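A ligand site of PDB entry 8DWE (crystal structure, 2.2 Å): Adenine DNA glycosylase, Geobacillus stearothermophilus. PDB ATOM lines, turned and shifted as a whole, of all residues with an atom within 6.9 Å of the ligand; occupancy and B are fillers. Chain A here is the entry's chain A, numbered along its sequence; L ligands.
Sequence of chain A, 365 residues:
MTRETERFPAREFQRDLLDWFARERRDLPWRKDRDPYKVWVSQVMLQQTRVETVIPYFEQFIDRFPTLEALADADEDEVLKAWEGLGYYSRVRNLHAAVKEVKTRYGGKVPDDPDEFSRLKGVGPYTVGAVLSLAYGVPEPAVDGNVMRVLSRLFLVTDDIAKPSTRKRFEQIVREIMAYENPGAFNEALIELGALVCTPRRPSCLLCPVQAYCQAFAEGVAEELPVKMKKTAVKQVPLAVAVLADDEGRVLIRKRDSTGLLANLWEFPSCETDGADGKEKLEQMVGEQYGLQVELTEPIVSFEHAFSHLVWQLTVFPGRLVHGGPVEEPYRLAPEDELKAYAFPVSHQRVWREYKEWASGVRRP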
ATOM      1  N   PHE A  13      -5.937  -4.380  -6.569  1.00  0.00           N
ATOM      2  CA  PHE A  13      -5.767  -4.266  -8.019  1.00  0.00           C
ATOM      3  C   PHE A  13      -4.299  -4.434  -8.421  1.00  0.00           C
ATOM      4  O   PHE A  13      -3.985  -5.226  -9.316  1.00  0.00           O
ATOM      5  CB  PHE A  13      -6.314  -2.908  -8.501  1.00  0.00           C
ATOM      6  CG  PHE A  13      -6.180  -2.675  -9.975  1.00  0.00           C
ATOM      7  CD1 PHE A  13      -7.054  -3.258 -10.878  1.00  0.00           C
ATOM      8  CD2 PHE A  13      -5.180  -1.844 -10.470  1.00  0.00           C
ATOM      9  CE1 PHE A  13      -6.931  -3.043 -12.260  1.00  0.00           C
ATOM     10  CE2 PHE A  13      -5.052  -1.632 -11.876  1.00  0.00           C
ATOM     11  CZ  PHE A  13      -5.941  -2.241 -12.762  1.00  0.00           C
ATOM     12  N   ARG A 149      -7.777   2.647 -23.264  1.00  0.00           N
ATOM     13  CA  ARG A 149      -8.821   1.635 -23.479  1.00  0.00           C
ATOM     14  C   ARG A 149      -9.107   0.861 -22.190  1.00  0.00           C
ATOM     15  O   ARG A 149     -10.264   0.783 -21.739  1.00  0.00           O
ATOM     16  CB  ARG A 149      -8.345   0.709 -24.593  1.00  0.00           C
ATOM     17  CG  ARG A 149      -9.023  -0.646 -24.604  1.00  0.00           C
ATOM     18  CD  ARG A 149      -8.927  -1.297 -25.972  1.00  0.00           C
ATOM     19  NE  ARG A 149      -7.780  -0.826 -26.743  1.00  0.00           N
ATOM     20  CZ  ARG A 149      -6.557  -1.326 -26.647  1.00  0.00           C
ATOM     21  NH1 ARG A 149      -6.277  -2.313 -25.812  1.00  0.00           N
ATOM     22  NH2 ARG A 149      -5.595  -0.851 -27.435  1.00  0.00           N
ATOM     23  N   VAL A 150      -8.073   0.300 -21.574  1.00  0.00           N
ATOM     24  CA  VAL A 150      -8.190  -0.379 -20.282  1.00  0.00           C
ATOM     25  C   VAL A 150      -8.865   0.510 -19.237  1.00  0.00           C
ATOM     26  O   VAL A 150      -9.762   0.069 -18.516  1.00  0.00           O
ATOM     27  CB  VAL A 150      -6.799  -0.831 -19.819  1.00  0.00           C
ATOM     28  CG1 VAL A 150      -6.804  -1.231 -18.349  1.00  0.00           C
ATOM     29  CG2 VAL A 150      -6.276  -1.942 -20.716  1.00  0.00           C
ATOM     30  N   ARG A 153     -12.592   1.185 -19.590  1.00  0.00           N
ATOM     31  CA  ARG A 153     -13.387   0.003 -19.270  1.00  0.00           C
ATOM     32  C   ARG A 153     -13.420  -0.287 -17.772  1.00  0.00           C
ATOM     33  O   ARG A 153     -14.499  -0.461 -17.200  1.00  0.00           O
ATOM     34  CB  ARG A 153     -12.850  -1.196 -20.056  1.00  0.00           C
ATOM     35  CG  ARG A 153     -13.260  -1.221 -21.550  1.00  0.00           C
ATOM     36  CD  ARG A 153     -12.383  -2.157 -22.382  1.00  0.00           C
ATOM     37  NE  ARG A 153     -12.768  -2.209 -23.789  1.00  0.00           N
ATOM     38  CZ  ARG A 153     -12.119  -2.907 -24.714  1.00  0.00           C
ATOM     39  NH1 ARG A 153     -10.982  -3.542 -24.444  1.00  0.00           N
ATOM     40  NH2 ARG A 153     -12.618  -2.980 -25.948  1.00  0.00           N
ATOM     41  N   LEU A 154     -12.249  -0.321 -17.114  1.00  0.00           N
ATOM     42  CA  LEU A 154     -12.225  -0.461 -15.664  1.00  0.00           C
ATOM     43  C   LEU A 154     -13.137   0.537 -14.990  1.00  0.00           C
ATOM     44  O   LEU A 154     -13.914   0.181 -14.115  1.00  0.00           O
ATOM     45  CB  LEU A 154     -10.805  -0.295 -15.138  1.00  0.00           C
ATOM     46  CG  LEU A 154      -9.890  -1.487 -15.481  1.00  0.00           C
ATOM     47  CD1 LEU A 154      -8.486  -1.100 -15.086  1.00  0.00           C
ATOM     48  CD2 LEU A 154     -10.276  -2.821 -14.807  1.00  0.00           C
ATOM     49  N   LEU A 193      -1.508  -5.206 -20.492  1.00  0.00           N
ATOM     50  CA  LEU A 193      -2.866  -5.729 -20.404  1.00  0.00           C
ATOM     51  C   LEU A 193      -3.687  -5.307 -21.616  1.00  0.00           C
ATOM     52  O   LEU A 193      -4.437  -6.107 -22.177  1.00  0.00           O
ATOM     53  CB  LEU A 193      -3.514  -5.248 -19.105  1.00  0.00           C
ATOM     54  CG  LEU A 193      -4.906  -5.722 -18.828  1.00  0.00           C
ATOM     55  CD1 LEU A 193      -4.875  -7.176 -18.517  1.00  0.00           C
ATOM     56  CD2 LEU A 193      -5.514  -4.930 -17.673  1.00  0.00           C
ATOM     57  N   VAL A 197      -4.722  -8.718 -23.544  1.00  0.00           N
ATOM     58  CA  VAL A 197      -5.980  -9.209 -22.999  1.00  0.00           C
ATOM     59  C   VAL A 197      -7.118  -8.251 -23.314  1.00  0.00           C
ATOM     60  O   VAL A 197      -8.102  -8.626 -23.955  1.00  0.00           O
ATOM     61  CB  VAL A 197      -5.834  -9.432 -21.484  1.00  0.00           C
ATOM     62  CG1 VAL A 197      -7.169  -9.847 -20.840  1.00  0.00           C
ATOM     63  CG2 VAL A 197      -4.733 -10.452 -21.228  1.00  0.00           C
ATOM     64  N   CYS A 198      -7.008  -6.998 -22.864  1.00  0.00           N
ATOM     65  CA  CYS A 198      -8.090  -6.008 -22.996  1.00  0.00           C
ATOM     66  C   CYS A 198      -7.969  -5.285 -24.347  1.00  0.00           C
ATOM     67  O   CYS A 198      -7.703  -4.100 -24.434  1.00  0.00           O
ATOM     68  CB  CYS A 198      -8.052  -5.034 -21.836  1.00  0.00           C
ATOM     69  SG  CYS A 198      -9.364  -3.899 -21.734  1.00  0.00           S
ATOM     70  N   THR A 199      -8.196  -6.054 -25.426  1.00  0.00           N
ATOM     71  CA  THR A 199      -7.917  -5.649 -26.789  1.00  0.00           C
ATOM     72  C   THR A 199      -9.065  -4.858 -27.408  1.00  0.00           C
ATOM     73  O   THR A 199     -10.206  -4.853 -26.909  1.00  0.00           O
ATOM     74  CB  THR A 199      -7.608  -6.893 -27.644  1.00  0.00           C
ATOM     75  OG1 THR A 199      -8.740  -7.773 -27.651  1.00  0.00           O
ATOM     76  CG2 THR A 199      -6.359  -7.636 -27.087  1.00  0.00           C
ATOM     77  N   PRO A 203     -12.426  -8.307 -26.309  1.00  0.00           N
ATOM     78  CA  PRO A 203     -11.494  -8.463 -25.177  1.00  0.00           C
ATOM     79  C   PRO A 203     -11.682  -9.798 -24.459  1.00  0.00           C
ATOM     80  O   PRO A 203     -12.797 -10.311 -24.353  1.00  0.00           O
ATOM     81  CB  PRO A 203     -11.850  -7.276 -24.261  1.00  0.00           C
ATOM     82  CG  PRO A 203     -13.251  -6.861 -24.672  1.00  0.00           C
ATOM     83  CD  PRO A 203     -13.346  -7.162 -26.137  1.00  0.00           C
ATOM     84  N   SER A 204     -10.577 -10.336 -23.946  1.00  0.00           N
ATOM     85  CA  SER A 204     -10.527 -11.647 -23.276  1.00  0.00           C
ATOM     86  C   SER A 204     -10.872 -11.539 -21.789  1.00  0.00           C
ATOM     87  O   SER A 204     -10.087 -11.971 -20.958  1.00  0.00           O
ATOM     88  CB  SER A 204      -9.145 -12.264 -23.447  1.00  0.00           C
ATOM     89  OG  SER A 204      -8.710 -12.263 -24.813  1.00  0.00           O
ATOM     90  N   CYS A 205     -12.020 -10.952 -21.447  1.00  0.00           N
ATOM     91  CA  CYS A 205     -12.349 -10.739 -20.045  1.00  0.00           C
ATOM     92  C   CYS A 205     -12.269 -11.995 -19.179  1.00  0.00           C
ATOM     93  O   CYS A 205     -12.103 -11.900 -17.958  1.00  0.00           O
ATOM     94  CB  CYS A 205     -13.760 -10.171 -19.940  1.00  0.00           C
ATOM     95  SG  CYS A 205     -14.086  -8.832 -21.026  1.00  0.00           S
ATOM     96  N   LEU A 206     -12.439 -13.175 -19.756  1.00  0.00           N
ATOM     97  CA  LEU A 206     -12.459 -14.392 -18.954  1.00  0.00           C
ATOM     98  C   LEU A 206     -11.058 -14.867 -18.579  1.00  0.00           C
ATOM     99  O   LEU A 206     -10.910 -15.585 -17.584  1.00  0.00           O
ATOM    100  CB  LEU A 206     -13.197 -15.502 -19.692  1.00  0.00           C
ATOM    101  CG  LEU A 206     -14.681 -15.260 -20.007  1.00  0.00           C
ATOM    102  CD1 LEU A 206     -15.153 -16.373 -20.917  1.00  0.00           C
ATOM    103  CD2 LEU A 206     -15.510 -15.153 -18.728  1.00  0.00           C
ATOM    104  N   LEU A 207     -10.050 -14.507 -19.363  1.00  0.00           N
ATOM    105  CA  LEU A 207      -8.645 -14.642 -18.999  1.00  0.00           C
ATOM    106  C   LEU A 207      -8.074 -13.386 -18.337  1.00  0.00           C
ATOM    107  O   LEU A 207      -6.843 -13.230 -18.291  1.00  0.00           O
ATOM    108  CB  LEU A 207      -7.790 -14.915 -20.229  1.00  0.00           C
ATOM    109  CG  LEU A 207      -8.233 -15.987 -21.201  1.00  0.00           C
ATOM    110  CD1 LEU A 207      -7.357 -15.906 -22.441  1.00  0.00           C
ATOM    111  CD2 LEU A 207      -8.139 -17.344 -20.551  1.00  0.00           C
ATOM    112  N   CYS A 208      -8.962 -12.452 -17.861  1.00  0.00           N
ATOM    113  CA  CYS A 208      -8.423 -11.174 -17.408  1.00  0.00           C
ATOM    114  C   CYS A 208      -8.087 -11.235 -15.934  1.00  0.00           C
ATOM    115  O   CYS A 208      -8.960 -11.523 -15.109  1.00  0.00           O
ATOM    116  CB  CYS A 208      -9.400 -10.051 -17.665  1.00  0.00           C
ATOM    117  SG  CYS A 208      -8.697  -8.514 -17.136  1.00  0.00           S
ATOM    118  N   PRO A 209      -6.861 -10.902 -15.558  1.00  0.00           N
ATOM    119  CA  PRO A 209      -6.516 -10.903 -14.127  1.00  0.00           C
ATOM    120  C   PRO A 209      -7.200  -9.851 -13.285  1.00  0.00           C
ATOM    121  O   PRO A 209      -7.087  -9.960 -12.064  1.00  0.00           O
ATOM    122  CB  PRO A 209      -5.018 -10.638 -14.124  1.00  0.00           C
ATOM    123  CG  PRO A 209      -4.818  -9.780 -15.384  1.00  0.00           C
ATOM    124  CD  PRO A 209      -5.832 -10.263 -16.385  1.00  0.00           C
ATOM    125  N   VAL A 210      -7.839  -8.834 -13.858  1.00  0.00           N
ATOM    126  CA  VAL A 210      -8.425  -7.771 -13.033  1.00  0.00           C
ATOM    127  C   VAL A 210      -9.916  -7.675 -13.321  1.00  0.00           C
ATOM    128  O   VAL A 210     -10.548  -6.627 -13.116  1.00  0.00           O
ATOM    129  CB  VAL A 210      -7.741  -6.397 -13.248  1.00  0.00           C
ATOM    130  CG1 VAL A 210      -6.308  -6.436 -12.710  1.00  0.00           C
ATOM    131  CG2 VAL A 210      -7.695  -6.016 -14.688  1.00  0.00           C
ATOM    132  N   GLN A 211     -10.493  -8.789 -13.778  1.00  0.00           N
ATOM    133  CA  GLN A 211     -11.925  -8.837 -14.073  1.00  0.00           C
ATOM    134  C   GLN A 211     -12.797  -8.399 -12.897  1.00  0.00           C
ATOM    135  O   GLN A 211     -13.871  -7.807 -13.097  1.00  0.00           O
ATOM    136  CB  GLN A 211     -12.261 -10.266 -14.486  1.00  0.00           C
ATOM    137  CG  GLN A 211     -13.638 -10.487 -14.989  1.00  0.00           C
ATOM    138  CD  GLN A 211     -14.008 -11.940 -14.830  1.00  0.00           C
ATOM    139  OE1 GLN A 211     -14.609 -12.345 -13.825  1.00  0.00           O
ATOM    140  NE2 GLN A 211     -13.593 -12.749 -15.793  1.00  0.00           N
ATOM    141  N   ALA A 212     -12.377  -8.687 -11.667  1.00  0.00           N
ATOM    142  CA  ALA A 212     -13.227  -8.380 -10.523  1.00  0.00           C
ATOM    143  C   ALA A 212     -13.250  -6.898 -10.168  1.00  0.00           C
ATOM    144  O   ALA A 212     -14.044  -6.483  -9.327  1.00  0.00           O
ATOM    145  CB  ALA A 212     -12.768  -9.161  -9.303  1.00  0.00           C
ATOM    146  N   TYR A 213     -12.403  -6.090 -10.789  1.00  0.00           N
ATOM    147  CA  TYR A 213     -12.389  -4.646 -10.577  1.00  0.00           C
ATOM    148  C   TYR A 213     -12.951  -3.864 -11.745  1.00  0.00           C
ATOM    149  O   TYR A 213     -12.943  -2.615 -11.701  1.00  0.00           O
ATOM    150  CB  TYR A 213     -10.951  -4.197 -10.330  1.00  0.00           C
ATOM    151  CG  TYR A 213     -10.156  -5.090  -9.413  1.00  0.00           C
ATOM    152  CD1 TYR A 213     -10.182  -4.938  -8.036  1.00  0.00           C
ATOM    153  CD2 TYR A 213      -9.360  -6.069  -9.934  1.00  0.00           C
ATOM    154  CE1 TYR A 213      -9.451  -5.782  -7.219  1.00  0.00           C
ATOM    155  CE2 TYR A 213      -8.631  -6.901  -9.135  1.00  0.00           C
ATOM    156  CZ  TYR A 213      -8.667  -6.760  -7.797  1.00  0.00           C
ATOM    157  OH  TYR A 213      -7.893  -7.643  -7.060  1.00  0.00           O
ATOM    158  N   CYS A 214     -13.423  -4.531 -12.800  1.00  0.00           N
ATOM    159  CA  CYS A 214     -13.777  -3.885 -14.053  1.00  0.00           C
ATOM    160  C   CYS A 214     -15.260  -3.555 -14.077  1.00  0.00           C
ATOM    161  O   CYS A 214     -16.109  -4.449 -13.936  1.00  0.00           O
ATOM    162  CB  CYS A 214     -13.447  -4.778 -15.235  1.00  0.00           C
ATOM    163  SG  CYS A 214     -13.825  -3.987 -16.804  1.00  0.00           S
ATOM    164  N   GLN A 215     -15.574  -2.272 -14.266  1.00  0.00           N
ATOM    165  CA  GLN A 215     -16.952  -1.813 -14.315  1.00  0.00           C
ATOM    166  C   GLN A 215     -17.622  -2.127 -15.648  1.00  0.00           C
ATOM    167  O   GLN A 215     -18.847  -2.312 -15.699  1.00  0.00           O
ATOM    168  CB  GLN A 215     -17.017  -0.304 -14.050  1.00  0.00           C
ATOM    169  CG  GLN A 215     -17.147   0.094 -12.598  1.00  0.00           C
ATOM    170  CD  GLN A 215     -17.518   1.573 -12.427  1.00  0.00           C
ATOM    171  OE1 GLN A 215     -18.655   1.986 -12.710  1.00  0.00           O
ATOM    172  NE2 GLN A 215     -16.565   2.368 -11.987  1.00  0.00           N
ATOM    173  N   ALA A 216     -16.882  -2.163 -16.754  1.00  0.00           N
ATOM    174  CA  ALA A 216     -17.551  -2.392 -18.027  1.00  0.00           C
ATOM    175  C   ALA A 216     -17.963  -3.852 -18.153  1.00  0.00           C
ATOM    176  O   ALA A 216     -19.035  -4.161 -18.663  1.00  0.00           O
ATOM    177  CB  ALA A 216     -16.688  -1.957 -19.212  1.00  0.00           C
ATOM    178  N   PHE A 217     -17.116  -4.755 -17.655  1.00  0.00           N
ATOM    179  CA  PHE A 217     -17.459  -6.167 -17.575  1.00  0.00           C
ATOM    180  C   PHE A 217     -18.751  -6.363 -16.801  1.00  0.00           C
ATOM    181  O   PHE A 217     -19.689  -7.008 -17.288  1.00  0.00           O
ATOM    182  CB  PHE A 217     -16.294  -6.922 -16.944  1.00  0.00           C
ATOM    183  CG  PHE A 217     -16.581  -8.366 -16.687  1.00  0.00           C
ATOM    184  CD1 PHE A 217     -16.679  -9.264 -17.745  1.00  0.00           C
ATOM    185  CD2 PHE A 217     -16.726  -8.824 -15.394  1.00  0.00           C
ATOM    186  CE1 PHE A 217     -16.939 -10.597 -17.504  1.00  0.00           C
ATOM    187  CE2 PHE A 217     -16.986 -10.171 -15.152  1.00  0.00           C
ATOM    188  CZ  PHE A 217     -17.088 -11.049 -16.217  1.00  0.00           C
ATOM    189  N   ALA A 222     -18.263  -3.433 -22.438  1.00  0.00           N
ATOM    190  CA  ALA A 222     -16.826  -3.338 -22.720  1.00  0.00           C
ATOM    191  C   ALA A 222     -16.534  -3.016 -24.188  1.00  0.00           C
ATOM    192  O   ALA A 222     -15.737  -2.124 -24.497  1.00  0.00           O
ATOM    193  CB  ALA A 222     -16.141  -4.637 -22.320  1.00  0.00           C
ATOM    194  N   GLU A 223     -17.127  -3.778 -25.096  1.00  0.00           N
ATOM    195  CA  GLU A 223     -16.798  -3.630 -26.517  1.00  0.00           C
ATOM    196  C   GLU A 223     -17.251  -2.306 -27.099  1.00  0.00           C
ATOM    197  O   GLU A 223     -16.867  -1.973 -28.230  1.00  0.00           O
ATOM    198  CB  GLU A 223     -17.415  -4.810 -27.279  1.00  0.00           C
ATOM    199  CG  GLU A 223     -16.729  -6.134 -26.977  1.00  0.00           C
ATOM    200  CD  GLU A 223     -17.611  -7.351 -27.215  1.00  0.00           C
ATOM    201  OE1 GLU A 223     -18.841  -7.207 -27.386  1.00  0.00           O
ATOM    202  OE2 GLU A 223     -17.067  -8.477 -27.227  1.00  0.00           O
HETATM  203 FE1  LIG L   1     -10.289  -7.113 -18.231  1.00  0.00          FE
HETATM  204 FE2  LIG L   1     -12.407  -7.296 -19.987  1.00  0.00          FE
HETATM  205 FE3  LIG L   1     -10.613  -5.303 -20.182  1.00  0.00          FE
HETATM  206 FE4  LIG L   1     -12.315  -5.364 -18.079  1.00  0.00          FE
HETATM  207  S1  LIG L   1     -12.877  -5.127 -20.309  1.00  0.00           S
HETATM  208  S2  LIG L   1     -10.113  -4.889 -18.001  1.00  0.00           S
HETATM  209  S3  LIG L   1     -12.428  -7.584 -17.714  1.00  0.00           S
HETATM  210  S4  LIG L   1     -10.231  -7.546 -20.514  1.00  0.00           S
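Merely in contact with the ligand: Arg 153, Leu 154, Val 197, Gln 211, Phe 217 and Ala 222.
Hydrophobic or aromatic side chains within 4 Å of the ligand: Leu 154, Val 197, Phe 217 and Ala 222.
Of the 26 residues printed, 10 come within 4 Å of the ligand.
The nearest printed residue that does not touch the ligand is Pro 203 (4.1 Å).
FE1 of the ligand is bound by SG of Cys 208, 2.4 Å away.
The side-chain sulfur of Cys 214 is bound to an iron atom (FE4) of the ligand (2.4 Å).
FE3 of the ligand is bound by SG of Cys 198 (2.4 Å).
SG of Cys 205 is bound to FE2 of the ligand.
The side-chain sulfur (SG) of Cys 208 sits close to the backbone NH (N) of Val 210 (3.4 Å).
The backbone NH of Phe 217 lies close to the side-chain sulfur of Cys 214 (3.5 Å).
SG of Cys 214 sits close to N of Ala 216, 3.6 Å away.
NE2 of Gln 211 is in hydrogen-bond range of O of Cys 205 (2.8 Å).
The guanidinium group (NE) of Arg 153 is in hydrogen-bond range of the backbone carbonyl oxygen (O) of Ala 222, at 3.1 Å.
The backbone NH (N) of Ala 216 is in hydrogen-bond range of the backbone carbonyl oxygen (O) of Arg 153, at 3.0 Å.
The backbone carbonyl oxygen (O) of Leu 154 is in hydrogen-bond range of the backbone NH (N) of Gln 215 (3.0 Å).
O of Val 197 lies within hydrogen-bond range of N of Ser 204 (3.0 Å).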
